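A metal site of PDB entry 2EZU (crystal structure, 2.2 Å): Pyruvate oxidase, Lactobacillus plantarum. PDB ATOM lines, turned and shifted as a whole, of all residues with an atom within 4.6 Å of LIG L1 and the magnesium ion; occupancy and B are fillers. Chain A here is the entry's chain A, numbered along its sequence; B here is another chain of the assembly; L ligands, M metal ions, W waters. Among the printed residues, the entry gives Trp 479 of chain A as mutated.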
ATOM      1  N   ASN A  92       5.973 -12.346   4.461  1.00  0.00           N
ATOM      2  CA  ASN A  92       4.759 -11.530   4.188  1.00  0.00           C
ATOM      3  C   ASN A  92       4.948 -10.079   4.497  1.00  0.00           C
ATOM      4  O   ASN A  92       4.406  -9.216   3.781  1.00  0.00           O
ATOM      5  CB  ASN A  92       3.487 -12.076   4.849  1.00  0.00           C
ATOM      6  CG  ASN A  92       2.845 -13.168   4.023  1.00  0.00           C
ATOM      7  OD1 ASN A  92       3.529 -14.114   3.629  1.00  0.00           O
ATOM      8  ND2 ASN A  92       1.537 -13.040   3.722  1.00  0.00           N
ATOM      9  N   VAL A 394      -6.982  -6.267   6.275  1.00  0.00           N
ATOM     10  CA  VAL A 394      -7.276  -6.409   4.857  1.00  0.00           C
ATOM     11  C   VAL A 394      -8.545  -7.243   4.663  1.00  0.00           C
ATOM     12  O   VAL A 394      -8.674  -8.357   5.194  1.00  0.00           O
ATOM     13  CB  VAL A 394      -6.065  -7.093   4.125  1.00  0.00           C
ATOM     14  CG1 VAL A 394      -6.456  -7.603   2.742  1.00  0.00           C
ATOM     15  CG2 VAL A 394      -4.879  -6.139   4.044  1.00  0.00           C
ATOM     16  N   GLY A 395      -9.476  -6.710   3.874  1.00  0.00           N
ATOM     17  CA  GLY A 395     -10.775  -7.344   3.697  1.00  0.00           C
ATOM     18  C   GLY A 395     -11.873  -6.267   3.652  1.00  0.00           C
ATOM     19  O   GLY A 395     -11.617  -5.133   3.218  1.00  0.00           O
ATOM     20  N   ASP A 396     -13.078  -6.631   4.114  1.00  0.00           N
ATOM     21  CA  ASP A 396     -14.195  -5.665   4.143  1.00  0.00           C
ATOM     22  C   ASP A 396     -13.861  -4.395   4.924  1.00  0.00           C
ATOM     23  O   ASP A 396     -14.403  -3.347   4.624  1.00  0.00           O
ATOM     24  CB  ASP A 396     -15.456  -6.265   4.749  1.00  0.00           C
ATOM     25  CG  ASP A 396     -16.323  -7.009   3.743  1.00  0.00           C
ATOM     26  OD1 ASP A 396     -16.074  -6.937   2.526  1.00  0.00           O
ATOM     27  OD2 ASP A 396     -17.305  -7.661   4.196  1.00  0.00           O
ATOM     28  N   ILE A 397     -12.993  -4.497   5.934  1.00  0.00           N
ATOM     29  CA  ILE A 397     -12.610  -3.340   6.753  1.00  0.00           C
ATOM     30  C   ILE A 397     -11.994  -2.189   5.926  1.00  0.00           C
ATOM     31  O   ILE A 397     -12.172  -1.027   6.268  1.00  0.00           O
ATOM     32  CB  ILE A 397     -11.671  -3.710   7.951  1.00  0.00           C
ATOM     33  CG1 ILE A 397     -11.482  -2.480   8.861  1.00  0.00           C
ATOM     34  CG2 ILE A 397     -10.279  -4.259   7.471  1.00  0.00           C
ATOM     35  CD1 ILE A 397     -12.792  -1.921   9.492  1.00  0.00           C
ATOM     36  N   ALA A 420      -1.274  -6.344  -0.014  1.00  0.00           N
ATOM     37  CA  ALA A 420      -2.572  -6.573   0.630  1.00  0.00           C
ATOM     38  C   ALA A 420      -2.537  -7.888   1.434  1.00  0.00           C
ATOM     39  O   ALA A 420      -3.444  -8.730   1.314  1.00  0.00           O
ATOM     40  CB  ALA A 420      -3.669  -6.624  -0.417  1.00  0.00           C
ATOM     41  N   THR A 421      -1.481  -8.064   2.234  1.00  0.00           N
ATOM     42  CA  THR A 421      -1.436  -9.171   3.187  1.00  0.00           C
ATOM     43  C   THR A 421      -2.296  -8.960   4.419  1.00  0.00           C
ATOM     44  O   THR A 421      -2.173  -7.951   5.138  1.00  0.00           O
ATOM     45  CB  THR A 421       0.021  -9.546   3.623  1.00  0.00           C
ATOM     46  OG1 THR A 421      -0.029 -10.662   4.516  1.00  0.00           O
ATOM     47  CG2 THR A 421       0.769  -8.353   4.343  1.00  0.00           C
ATOM     48  N   MET A 422      -3.178  -9.931   4.681  1.00  0.00           N
ATOM     49  CA  MET A 422      -3.945 -10.019   5.906  1.00  0.00           C
ATOM     50  C   MET A 422      -3.012 -10.170   7.103  1.00  0.00           C
ATOM     51  O   MET A 422      -1.890 -10.674   6.957  1.00  0.00           O
ATOM     52  CB  MET A 422      -4.867 -11.237   5.833  1.00  0.00           C
ATOM     53  CG  MET A 422      -6.091 -11.089   4.893  1.00  0.00           C
ATOM     54  SD  MET A 422      -6.908 -12.680   4.619  1.00  0.00           S
ATOM     55  CE  MET A 422      -7.553 -13.006   6.274  1.00  0.00           C
ATOM     56  N   GLY A 446     -10.666  -7.490  10.383  1.00  0.00           N
ATOM     57  CA  GLY A 446     -11.646  -8.591  10.268  1.00  0.00           C
ATOM     58  C   GLY A 446     -11.181  -9.773  11.099  1.00  0.00           C
ATOM     59  O   GLY A 446      -9.995  -9.846  11.510  1.00  0.00           O
ATOM     60  N   ASP A 447     -12.106 -10.706  11.353  1.00  0.00           N
ATOM     61  CA  ASP A 447     -11.790 -11.898  12.121  1.00  0.00           C
ATOM     62  C   ASP A 447     -10.798 -12.819  11.408  1.00  0.00           C
ATOM     63  O   ASP A 447      -9.928 -13.405  12.063  1.00  0.00           O
ATOM     64  CB  ASP A 447     -13.047 -12.674  12.565  1.00  0.00           C
ATOM     65  CG  ASP A 447     -14.026 -12.990  11.429  1.00  0.00           C
ATOM     66  OD1 ASP A 447     -13.836 -12.666  10.233  1.00  0.00           O
ATOM     67  OD2 ASP A 447     -15.073 -13.591  11.770  1.00  0.00           O
ATOM     68  N   GLY A 448     -10.923 -12.921  10.081  1.00  0.00           N
ATOM     69  CA  GLY A 448      -9.941 -13.666   9.288  1.00  0.00           C
ATOM     70  C   GLY A 448      -8.521 -13.143   9.443  1.00  0.00           C
ATOM     71  O   GLY A 448      -7.598 -13.910   9.684  1.00  0.00           O
ATOM     72  N   GLY A 449      -8.336 -11.829   9.283  1.00  0.00           N
ATOM     73  CA  GLY A 449      -6.986 -11.239   9.397  1.00  0.00           C
ATOM     74  C   GLY A 449      -6.452 -11.177  10.821  1.00  0.00           C
ATOM     75  O   GLY A 449      -5.270 -11.440  11.050  1.00  0.00           O
ATOM     76  N   MET A 452      -4.896 -14.532  11.880  1.00  0.00           N
ATOM     77  CA  MET A 452      -3.566 -14.839  11.380  1.00  0.00           C
ATOM     78  C   MET A 452      -2.406 -14.355  12.266  1.00  0.00           C
ATOM     79  O   MET A 452      -1.363 -15.027  12.324  1.00  0.00           O
ATOM     80  CB  MET A 452      -3.444 -14.275   9.972  1.00  0.00           C
ATOM     81  CG  MET A 452      -4.281 -15.111   8.988  1.00  0.00           C
ATOM     82  SD  MET A 452      -4.084 -14.533   7.310  1.00  0.00           S
ATOM     83  CE  MET A 452      -4.933 -15.830   6.364  1.00  0.00           C
ATOM     84  N   PHE A 472     -13.901  -7.303  13.667  1.00  0.00           N
ATOM     85  CA  PHE A 472     -15.202  -7.398  13.005  1.00  0.00           C
ATOM     86  C   PHE A 472     -15.499  -8.852  12.676  1.00  0.00           C
ATOM     87  O   PHE A 472     -15.053  -9.354  11.628  1.00  0.00           O
ATOM     88  CB  PHE A 472     -15.213  -6.523  11.737  1.00  0.00           C
ATOM     89  CG  PHE A 472     -15.048  -5.037  12.028  1.00  0.00           C
ATOM     90  CD1 PHE A 472     -13.803  -4.516  12.414  1.00  0.00           C
ATOM     91  CD2 PHE A 472     -16.137  -4.154  11.926  1.00  0.00           C
ATOM     92  CE1 PHE A 472     -13.644  -3.143  12.726  1.00  0.00           C
ATOM     93  CE2 PHE A 472     -15.983  -2.782  12.208  1.00  0.00           C
ATOM     94  CZ  PHE A 472     -14.733  -2.278  12.610  1.00  0.00           C
ATOM     95  N   ASN A 474     -17.579 -11.591  11.495  1.00  0.00           N
ATOM     96  CA  ASN A 474     -18.676 -12.082  10.682  1.00  0.00           C
ATOM     97  C   ASN A 474     -18.634 -13.602  10.471  1.00  0.00           C
ATOM     98  O   ASN A 474     -19.499 -14.151   9.796  1.00  0.00           O
ATOM     99  CB  ASN A 474     -18.779 -11.314   9.355  1.00  0.00           C
ATOM    100  CG  ASN A 474     -17.486 -11.272   8.605  1.00  0.00           C
ATOM    101  OD1 ASN A 474     -16.538 -11.948   8.966  1.00  0.00           O
ATOM    102  ND2 ASN A 474     -17.459 -10.529   7.502  1.00  0.00           N
ATOM    103  N   GLN A 476     -16.757 -15.014   8.567  1.00  0.00           N
ATOM    104  CA  GLN A 476     -16.532 -15.202   7.129  1.00  0.00           C
ATOM    105  C   GLN A 476     -15.243 -14.541   6.708  1.00  0.00           C
ATOM    106  O   GLN A 476     -14.755 -13.624   7.364  1.00  0.00           O
ATOM    107  CB  GLN A 476     -17.685 -14.567   6.309  1.00  0.00           C
ATOM    108  CG  GLN A 476     -19.097 -15.060   6.651  1.00  0.00           C
ATOM    109  CD  GLN A 476     -20.217 -14.178   6.048  1.00  0.00           C
ATOM    110  OE1 GLN A 476     -21.340 -14.607   5.906  1.00  0.00           O
ATOM    111  NE2 GLN A 476     -19.883 -12.947   5.687  1.00  0.00           N
ATOM    112  N   TYR A 477     -14.714 -14.983   5.573  1.00  0.00           N
ATOM    113  CA  TYR A 477     -13.880 -14.161   4.733  1.00  0.00           C
ATOM    114  C   TYR A 477     -14.859 -13.429   3.821  1.00  0.00           C
ATOM    115  O   TYR A 477     -15.057 -13.843   2.662  1.00  0.00           O
ATOM    116  CB  TYR A 477     -12.930 -15.031   3.876  1.00  0.00           C
ATOM    117  CG  TYR A 477     -11.949 -15.842   4.676  1.00  0.00           C
ATOM    118  CD1 TYR A 477     -11.083 -15.204   5.592  1.00  0.00           C
ATOM    119  CD2 TYR A 477     -11.870 -17.237   4.520  1.00  0.00           C
ATOM    120  CE1 TYR A 477     -10.184 -15.950   6.367  1.00  0.00           C
ATOM    121  CE2 TYR A 477     -10.967 -17.978   5.274  1.00  0.00           C
ATOM    122  CZ  TYR A 477     -10.131 -17.324   6.205  1.00  0.00           C
ATOM    123  OH  TYR A 477      -9.244 -18.054   6.934  1.00  0.00           O
ATOM    124  N   GLY A 478     -15.476 -12.372   4.330  1.00  0.00           N
ATOM    125  CA  GLY A 478     -16.591 -11.709   3.604  1.00  0.00           C
ATOM    126  C   GLY A 478     -16.166 -11.139   2.249  1.00  0.00           C
ATOM    127  O   GLY A 478     -16.905 -11.297   1.247  1.00  0.00           O
ATOM    128  N   TRP A 479     -14.999 -10.512   2.200  1.00  0.00           N
ATOM    129  CA  TRP A 479     -14.456  -9.953   0.949  1.00  0.00           C
ATOM    130  C   TRP A 479     -14.456 -11.000  -0.155  1.00  0.00           C
ATOM    131  O   TRP A 479     -14.785 -10.691  -1.305  1.00  0.00           O
ATOM    132  CB  TRP A 479     -13.013  -9.480   1.183  1.00  0.00           C
ATOM    133  CG  TRP A 479     -12.404  -8.565   0.148  1.00  0.00           C
ATOM    134  CD1 TRP A 479     -11.403  -8.872  -0.727  1.00  0.00           C
ATOM    135  CD2 TRP A 479     -12.734  -7.184  -0.075  1.00  0.00           C
ATOM    136  NE1 TRP A 479     -11.081  -7.772  -1.488  1.00  0.00           N
ATOM    137  CE2 TRP A 479     -11.880  -6.717  -1.117  1.00  0.00           C
ATOM    138  CE3 TRP A 479     -13.674  -6.293   0.476  1.00  0.00           C
ATOM    139  CZ2 TRP A 479     -11.940  -5.397  -1.614  1.00  0.00           C
ATOM    140  CZ3 TRP A 479     -13.736  -4.986  -0.010  1.00  0.00           C
ATOM    141  CH2 TRP A 479     -12.870  -4.554  -1.056  1.00  0.00           C
ATOM    142  N   ILE A 480     -14.075 -12.225   0.198  1.00  0.00           N
ATOM    143  CA  ILE A 480     -13.993 -13.373  -0.745  1.00  0.00           C
ATOM    144  C   ILE A 480     -15.342 -14.038  -0.985  1.00  0.00           C
ATOM    145  O   ILE A 480     -15.612 -14.492  -2.112  1.00  0.00           O
ATOM    146  CB  ILE A 480     -12.954 -14.451  -0.243  1.00  0.00           C
ATOM    147  CG1 ILE A 480     -11.634 -13.772   0.189  1.00  0.00           C
ATOM    148  CG2 ILE A 480     -12.691 -15.578  -1.285  1.00  0.00           C
ATOM    149  CD1 ILE A 480     -11.002 -12.912  -0.916  1.00  0.00           C
ATOM    150  N   ILE B  32      -6.727 -21.440   1.765  1.00  0.00           N
ATOM    151  CA  ILE B  32      -7.623 -20.313   2.063  1.00  0.00           C
ATOM    152  C   ILE B  32      -7.941 -19.687   0.723  1.00  0.00           C
ATOM    153  O   ILE B  32      -7.010 -19.507  -0.062  1.00  0.00           O
ATOM    154  CB  ILE B  32      -6.944 -19.276   3.017  1.00  0.00           C
ATOM    155  CG1 ILE B  32      -6.830 -19.858   4.441  1.00  0.00           C
ATOM    156  CG2 ILE B  32      -7.713 -17.911   2.987  1.00  0.00           C
ATOM    157  CD1 ILE B  32      -6.075 -19.011   5.488  1.00  0.00           C
ATOM    158  N   PRO B  33      -9.239 -19.442   0.418  1.00  0.00           N
ATOM    159  CA  PRO B  33      -9.592 -18.930  -0.938  1.00  0.00           C
ATOM    160  C   PRO B  33      -9.204 -17.457  -1.130  1.00  0.00           C
ATOM    161  O   PRO B  33      -8.832 -16.798  -0.175  1.00  0.00           O
ATOM    162  CB  PRO B  33     -11.122 -19.085  -0.996  1.00  0.00           C
ATOM    163  CG  PRO B  33     -11.548 -18.970   0.477  1.00  0.00           C
ATOM    164  CD  PRO B  33     -10.429 -19.630   1.270  1.00  0.00           C
ATOM    165  N   GLY B  34      -9.305 -16.972  -2.370  1.00  0.00           N
ATOM    166  CA  GLY B  34      -9.065 -15.567  -2.700  1.00  0.00           C
ATOM    167  C   GLY B  34      -9.569 -15.389  -4.124  1.00  0.00           C
ATOM    168  O   GLY B  34      -9.742 -16.374  -4.830  1.00  0.00           O
ATOM    169  N   GLU B  59      -2.299 -19.890   5.936  1.00  0.00           N
ATOM    170  CA  GLU B  59      -1.828 -20.800   4.878  1.00  0.00           C
ATOM    171  C   GLU B  59      -0.592 -21.612   5.231  1.00  0.00           C
ATOM    172  O   GLU B  59      -0.427 -22.679   4.667  1.00  0.00           O
ATOM    173  CB  GLU B  59      -1.649 -20.114   3.514  1.00  0.00           C
ATOM    174  CG  GLU B  59      -2.905 -19.444   2.981  1.00  0.00           C
ATOM    175  CD  GLU B  59      -3.078 -18.002   3.493  1.00  0.00           C
ATOM    176  OE1 GLU B  59      -2.434 -17.612   4.513  1.00  0.00           O
ATOM    177  OE2 GLU B  59      -3.847 -17.280   2.853  1.00  0.00           O
ATOM    178  N   SER B  82      -3.769 -18.058  -2.182  1.00  0.00           N
ATOM    179  CA  SER B  82      -4.099 -17.045  -3.201  1.00  0.00           C
ATOM    180  C   SER B  82      -2.841 -16.218  -3.593  1.00  0.00           C
ATOM    181  O   SER B  82      -1.787 -16.313  -2.931  1.00  0.00           O
ATOM    182  CB  SER B  82      -5.216 -16.134  -2.708  1.00  0.00           C
ATOM    183  OG  SER B  82      -4.876 -15.707  -1.403  1.00  0.00           O
ATOM    184  N   PRO B  85       0.285 -12.705  -0.868  1.00  0.00           N
ATOM    185  CA  PRO B  85       0.404 -13.117   0.525  1.00  0.00           C
ATOM    186  C   PRO B  85      -0.125 -14.530   0.874  1.00  0.00           C
ATOM    187  O   PRO B  85       0.324 -15.112   1.837  1.00  0.00           O
ATOM    188  CB  PRO B  85      -0.418 -12.046   1.280  1.00  0.00           C
ATOM    189  CG  PRO B  85      -1.357 -11.489   0.283  1.00  0.00           C
ATOM    190  CD  PRO B  85      -0.564 -11.500  -1.010  1.00  0.00           C
ATOM    191  N   GLY B  86      -1.071 -15.073   0.112  1.00  0.00           N
ATOM    192  CA  GLY B  86      -1.598 -16.417   0.401  1.00  0.00           C
ATOM    193  C   GLY B  86      -0.482 -17.438   0.209  1.00  0.00           C
ATOM    194  O   GLY B  86      -0.228 -18.277   1.071  1.00  0.00           O
ATOM    195  N   HIS B  89       2.734 -17.172   2.466  1.00  0.00           N
ATOM    196  CA  HIS B  89       2.445 -17.763   3.772  1.00  0.00           C
ATOM    197  C   HIS B  89       2.726 -19.274   3.807  1.00  0.00           C
ATOM    198  O   HIS B  89       2.883 -19.855   4.887  1.00  0.00           O
ATOM    199  CB  HIS B  89       0.976 -17.534   4.204  1.00  0.00           C
ATOM    200  CG  HIS B  89       0.771 -16.415   5.164  1.00  0.00           C
ATOM    201  ND1 HIS B  89      -0.489 -16.026   5.593  1.00  0.00           N
ATOM    202  CD2 HIS B  89       1.653 -15.589   5.793  1.00  0.00           C
ATOM    203  CE1 HIS B  89      -0.368 -15.031   6.448  1.00  0.00           C
ATOM    204  NE2 HIS B  89       0.918 -14.727   6.574  1.00  0.00           N
ATOM    205  N   PHE B 121      -3.603  -5.060  -8.816  1.00  0.00           N
ATOM    206  CA  PHE B 121      -3.727  -5.365  -7.405  1.00  0.00           C
ATOM    207  C   PHE B 121      -3.267  -6.787  -7.059  1.00  0.00           C
ATOM    208  O   PHE B 121      -3.697  -7.767  -7.709  1.00  0.00           O
ATOM    209  CB  PHE B 121      -5.202  -5.169  -7.005  1.00  0.00           C
ATOM    210  CG  PHE B 121      -5.494  -5.477  -5.572  1.00  0.00           C
ATOM    211  CD1 PHE B 121      -5.127  -4.601  -4.568  1.00  0.00           C
ATOM    212  CD2 PHE B 121      -6.114  -6.654  -5.226  1.00  0.00           C
ATOM    213  CE1 PHE B 121      -5.379  -4.884  -3.243  1.00  0.00           C
ATOM    214  CE2 PHE B 121      -6.387  -6.947  -3.879  1.00  0.00           C
ATOM    215  CZ  PHE B 121      -6.026  -6.049  -2.905  1.00  0.00           C
ATOM    216  N   GLN B 122      -2.426  -6.899  -6.019  1.00  0.00           N
ATOM    217  CA  GLN B 122      -1.750  -8.168  -5.619  1.00  0.00           C
ATOM    218  C   GLN B 122      -1.165  -8.945  -6.791  1.00  0.00           C
ATOM    219  O   GLN B 122      -1.126 -10.183  -6.749  1.00  0.00           O
ATOM    220  CB  GLN B 122      -2.705  -9.141  -4.885  1.00  0.00           C
ATOM    221  CG  GLN B 122      -3.044  -8.720  -3.531  1.00  0.00           C
ATOM    222  CD  GLN B 122      -3.914  -9.728  -2.808  1.00  0.00           C
ATOM    223  OE1 GLN B 122      -4.857 -10.278  -3.380  1.00  0.00           O
ATOM    224  NE2 GLN B 122      -3.622  -9.945  -1.546  1.00  0.00           N
HETATM  225  N1  LIG L   1      -4.180 -14.751   2.677  1.00  0.00           N
HETATM  226  C1  LIG L   1      -3.476 -13.644   3.035  1.00  0.00           C
HETATM  227  C2  LIG L   1      -2.321 -13.732   3.999  1.00  0.00           C
HETATM  228  N2  LIG L   1      -3.786 -12.434   2.523  1.00  0.00           N
HETATM  229  C3  LIG L   1      -4.804 -12.282   1.638  1.00  0.00           C
HETATM  230  N3  LIG L   1      -5.013 -11.028   1.166  1.00  0.00           N
HETATM  231  C4  LIG L   1      -5.584 -13.399   1.248  1.00  0.00           C
HETATM  232  C5  LIG L   1      -5.213 -14.644   1.817  1.00  0.00           C
HETATM  233  C6  LIG L   1      -6.773 -13.318   0.270  1.00  0.00           C
HETATM  234  N4  LIG L   1      -7.828 -12.445   0.871  1.00  0.00           N
HETATM  235  C7  LIG L   1      -8.044 -11.114   0.570  1.00  0.00           C
HETATM  236  S1  LIG L   1      -9.309 -10.415   1.563  1.00  0.00           S
HETATM  237  C8  LIG L   1      -9.587 -11.941   2.366  1.00  0.00           C
HETATM  238  C9  LIG L   1      -8.679 -12.923   1.865  1.00  0.00           C
HETATM  239  C10 LIG L   1      -8.682 -14.343   2.413  1.00  0.00           C
HETATM  240  C11 LIG L   1     -10.684 -12.024   3.403  1.00  0.00           C
HETATM  241  C12 LIG L   1     -10.463 -11.201   4.672  1.00  0.00           C
HETATM  242  O1  LIG L   1     -11.290 -11.807   5.671  1.00  0.00           O
HETATM  243  P1  LIG L   1     -11.595 -11.084   7.028  1.00  0.00           P
HETATM  244  O2  LIG L   1     -12.397  -9.748   6.571  1.00  0.00           O
HETATM  245  O3  LIG L   1     -12.525 -11.893   7.896  1.00  0.00           O
HETATM  246  O4  LIG L   1     -10.305 -10.589   7.624  1.00  0.00           O
HETATM  247  P2  LIG L   1     -13.961  -9.579   6.188  1.00  0.00           P
HETATM  248  O5  LIG L   1     -14.299  -8.355   7.037  1.00  0.00           O
HETATM  249  O6  LIG L   1     -13.954  -9.293   4.703  1.00  0.00           O
HETATM  250  O7  LIG L   1     -14.760 -10.801   6.561  1.00  0.00           O
HETATM  251  C13 LIG L   1      -7.429 -10.181  -0.460  1.00  0.00           C
HETATM  252  O8  LIG L   1      -6.627 -10.623  -1.274  1.00  0.00           O
HETATM  253  C14 LIG L   1      -7.904  -8.748  -0.617  1.00  0.00           C
HETATM  254  P1  LG2 L   2       1.294   4.419  -4.670  1.00  0.00           P
HETATM  255  O1  LG2 L   2       2.244   4.290  -3.498  1.00  0.00           O
HETATM  256  O2  LG2 L   2       1.069   3.206  -5.520  1.00  0.00           O
HETATM  257  O3  LG2 L   2       1.798   5.575  -5.669  1.00  0.00           O
HETATM  258  C1  LG2 L   2       2.260   6.846  -5.218  1.00  0.00           C
HETATM  259  C2  LG2 L   2       2.721   7.597  -6.442  1.00  0.00           C
HETATM  260  O4  LG2 L   2       3.158   8.887  -6.034  1.00  0.00           O
HETATM  261  C3  LG2 L   2       3.921   6.949  -7.132  1.00  0.00           C
HETATM  262  O5  LG2 L   2       3.628   6.911  -8.535  1.00  0.00           O
HETATM  263  C4  LG2 L   2       5.101   7.850  -6.792  1.00  0.00           C
HETATM  264  O6  LG2 L   2       6.049   7.960  -7.829  1.00  0.00           O
HETATM  265  C5  LG2 L   2       4.427   9.187  -6.662  1.00  0.00           C
HETATM  266  N1  LG2 L   2       5.099  10.171  -5.789  1.00  0.00           N
HETATM  267  C6  LG2 L   2       5.702   9.933  -4.593  1.00  0.00           C
HETATM  268  N2  LG2 L   2       6.123  11.105  -4.085  1.00  0.00           N
HETATM  269  C7  LG2 L   2       5.764  12.093  -4.975  1.00  0.00           C
HETATM  270  C8  LG2 L   2       5.939  13.474  -5.004  1.00  0.00           C
HETATM  271  N3  LG2 L   2       6.589  14.121  -3.976  1.00  0.00           N
HETATM  272  N4  LG2 L   2       5.443  14.180  -6.052  1.00  0.00           N
HETATM  273  C9  LG2 L   2       4.811  13.570  -7.078  1.00  0.00           C
HETATM  274  N5  LG2 L   2       4.628  12.233  -7.080  1.00  0.00           N
HETATM  275  C10 LG2 L   2       5.096  11.484  -6.042  1.00  0.00           C
HETATM  276  N6  LG2 L   2      -7.325   1.432  -3.815  1.00  0.00           N
HETATM  277  C11 LG2 L   2      -8.317   2.109  -4.460  1.00  0.00           C
HETATM  278  O7  LG2 L   2      -8.139   3.317  -4.702  1.00  0.00           O
HETATM  279  N7  LG2 L   2      -9.463   1.456  -4.835  1.00  0.00           N
HETATM  280  C12 LG2 L   2      -9.603   0.135  -4.541  1.00  0.00           C
HETATM  281  O8  LG2 L   2     -10.633  -0.465  -4.852  1.00  0.00           O
HETATM  282  C13 LG2 L   2      -8.597  -0.567  -3.860  1.00  0.00           C
HETATM  283  N8  LG2 L   2      -8.672  -1.901  -3.553  1.00  0.00           N
HETATM  284  C14 LG2 L   2      -7.986  -2.335  -2.459  1.00  0.00           C
HETATM  285  C15 LG2 L   2      -8.404  -3.441  -1.721  1.00  0.00           C
HETATM  286  C16 LG2 L   2      -7.707  -3.855  -0.592  1.00  0.00           C
HETATM  287  C17 LG2 L   2      -8.215  -5.074   0.152  1.00  0.00           C
HETATM  288  C18 LG2 L   2      -6.568  -3.142  -0.185  1.00  0.00           C
HETATM  289  C19 LG2 L   2      -5.725  -3.517   1.029  1.00  0.00           C
HETATM  290  C20 LG2 L   2      -6.143  -2.022  -0.943  1.00  0.00           C
HETATM  291  C21 LG2 L   2      -6.846  -1.609  -2.063  1.00  0.00           C
HETATM  292  N9  LG2 L   2      -6.472  -0.537  -2.822  1.00  0.00           N
HETATM  293  C22 LG2 L   2      -7.457   0.122  -3.488  1.00  0.00           C
HETATM  294  C23 LG2 L   2      -5.251   0.222  -2.528  1.00  0.00           C
HETATM  295  C24 LG2 L   2      -4.503   0.017  -3.896  1.00  0.00           C
HETATM  296  O9  LG2 L   2      -4.117  -1.350  -4.169  1.00  0.00           O
HETATM  297  C25 LG2 L   2      -3.256   0.878  -4.195  1.00  0.00           C
HETATM  298  O10 LG2 L   2      -2.197   0.659  -3.230  1.00  0.00           O
HETATM  299  C26 LG2 L   2      -3.618   2.376  -4.329  1.00  0.00           C
HETATM  300  O11 LG2 L   2      -4.808   2.624  -5.117  1.00  0.00           O
HETATM  301  C27 LG2 L   2      -2.444   3.146  -4.937  1.00  0.00           C
HETATM  302  O12 LG2 L   2      -2.443   4.372  -4.194  1.00  0.00           O
HETATM  303  P2  LG2 L   2      -1.442   5.591  -4.476  1.00  0.00           P
HETATM  304  O13 LG2 L   2      -1.314   5.826  -5.959  1.00  0.00           O
HETATM  305  O14 LG2 L   2      -1.953   6.660  -3.560  1.00  0.00           O
HETATM  306  O15 LG2 L   2      -0.076   4.941  -3.948  1.00  0.00           O
HETATM  307 MG    MG M   1     -14.421 -11.858   8.365  1.00  0.00          MG
HETATM  308  O   HOH W   1      -4.275 -13.024  -2.100  1.00  0.00           O
HETATM  309  O   HOH W   2     -12.080  -6.919   7.344  1.00  0.00           O
HETATM  310  O   HOH W   3      -9.596  -8.140   7.774  1.00  0.00           O
HETATM  311  O   HOH W   4     -16.288  -6.755   8.230  1.00  0.00           O
HETATM  312  O   HOH W   5     -14.362  -9.830   9.247  1.00  0.00           O
HETATM  313  O   HOH W   6      -8.981 -11.527  -3.209  1.00  0.00           O
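The backbone NH (N) of Asp 396 lies within hydrogen-bond range of an oxygen (O6) of LIG L1 (2.9 Å). N3 of LIG L1 is in hydrogen-bond range of O of Ala 420, at 2.8 Å. The backbone NH of Gly 449 sits at hydrogen-bond distance from an oxygen (O4) of LIG L1. An oxygen (O4) of LIG L1 is in hydrogen-bond range of the backbone NH (N) of Gly 448 (3.4 Å). O6 of LIG L1 lies within hydrogen-bond range of N of Gly 478. The side-chain amide oxygen (OE1) of Gln 122 of chain B lies close to an oxygen (O8) of LIG L1 (2.8 Å). N1 of LIG L1 lies within hydrogen-bond range of OE2 of Glu 59 of chain B. N of Met 422 sits at hydrogen-bond distance from N2 of LIG L1, at 3.4 Å. An oxygen (O6) of LIG L1 is in hydrogen-bond range of the backbone NH (N) of Trp 479 (3.0 Å).
Residues that only touch LIG L1: His 89 of chain B (3.3 Å), Val 394 (3.4 Å), Tyr 477 (3.4 Å), Ser 82 of chain B (3.4 Å), Pro 85 of chain B (3.4 Å), Ile 480 (3.5 Å), Pro 33 of chain B (3.6 Å), Gly 446 (3.6 Å), Ile 32 of chain B (3.7 Å), Gly 395 (3.8 Å), Gly 86 of chain B (3.8 Å), Met 452 (3.8 Å), Thr 421 (3.9 Å) and Asn 92 (3.9 Å). Along chain A the residues within 4 Å of LIG L1 span positions 92 to 480.
The magnesium ion is bound by O3 of LIG L1, at 2.0 Å. The magnesium ion is bound by O of Gln 476 (2.1 Å). The side-chain carboxylate (OD1) of Asp 447 binds the magnesium ion, at 2.1 Å. The magnesium ion is bound by O7 of LIG L1, 2.1 Å away. OD1 of Asn 474 is bound to the magnesium ion. Water W5 is bound to the magnesium ion (2.2 Å).
Within 4 Å of the magnesium ion: Asp 447, Asn 474 and Gln 476. Along chain A the residues within 4 Å of the magnesium ion span positions 447 to 476. The nearest printed residue that does not touch the magnesium ion is Gly 448 (4.04 Å).
The backbone NH of His 89 of chain B lies close to the side-chain amide oxygen of Asn 92. The side-chain carboxylate (OE1) of Glu 59 of chain B is in hydrogen-bond range of a ring nitrogen (ND1) of His 89 of chain B (2.7 Å). The backbone NH (N) of Asp 447 sits at hydrogen-bond distance from the backbone carbonyl oxygen (O) of Phe 472 (3.3 Å). The backbone carbonyl oxygen (O) of Pro 85 of chain B sits at hydrogen-bond distance from the side-chain amide nitrogen (ND2) of Asn 92, at 3.1 Å. OG1 of Thr 421 is in hydrogen-bond range of ND2 of Asn 92 (3.0 Å). The backbone carbonyl oxygen of Ala 420 is in hydrogen-bond range of the side-chain amide nitrogen of Gln 122 of chain B, at 3.1 Å.
Water W5 lies within hydrogen-bond range of O of Phe 472, O5 of LIG L1 and N of Asp 447. Water W3 lies within hydrogen-bond range of an oxygen (O4) of LIG L1 (2.6 Å), the backbone carbonyl oxygen (O) of Val 394 (2.7 Å) and the backbone NH (N) of Gly 446 (2.9 Å). Water W1 lies within hydrogen-bond range of the side-chain hydroxyl of Ser 82 of chain B, the side-chain amide oxygen of Gln 122 of chain B and an oxygen (O8) of LIG L1.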
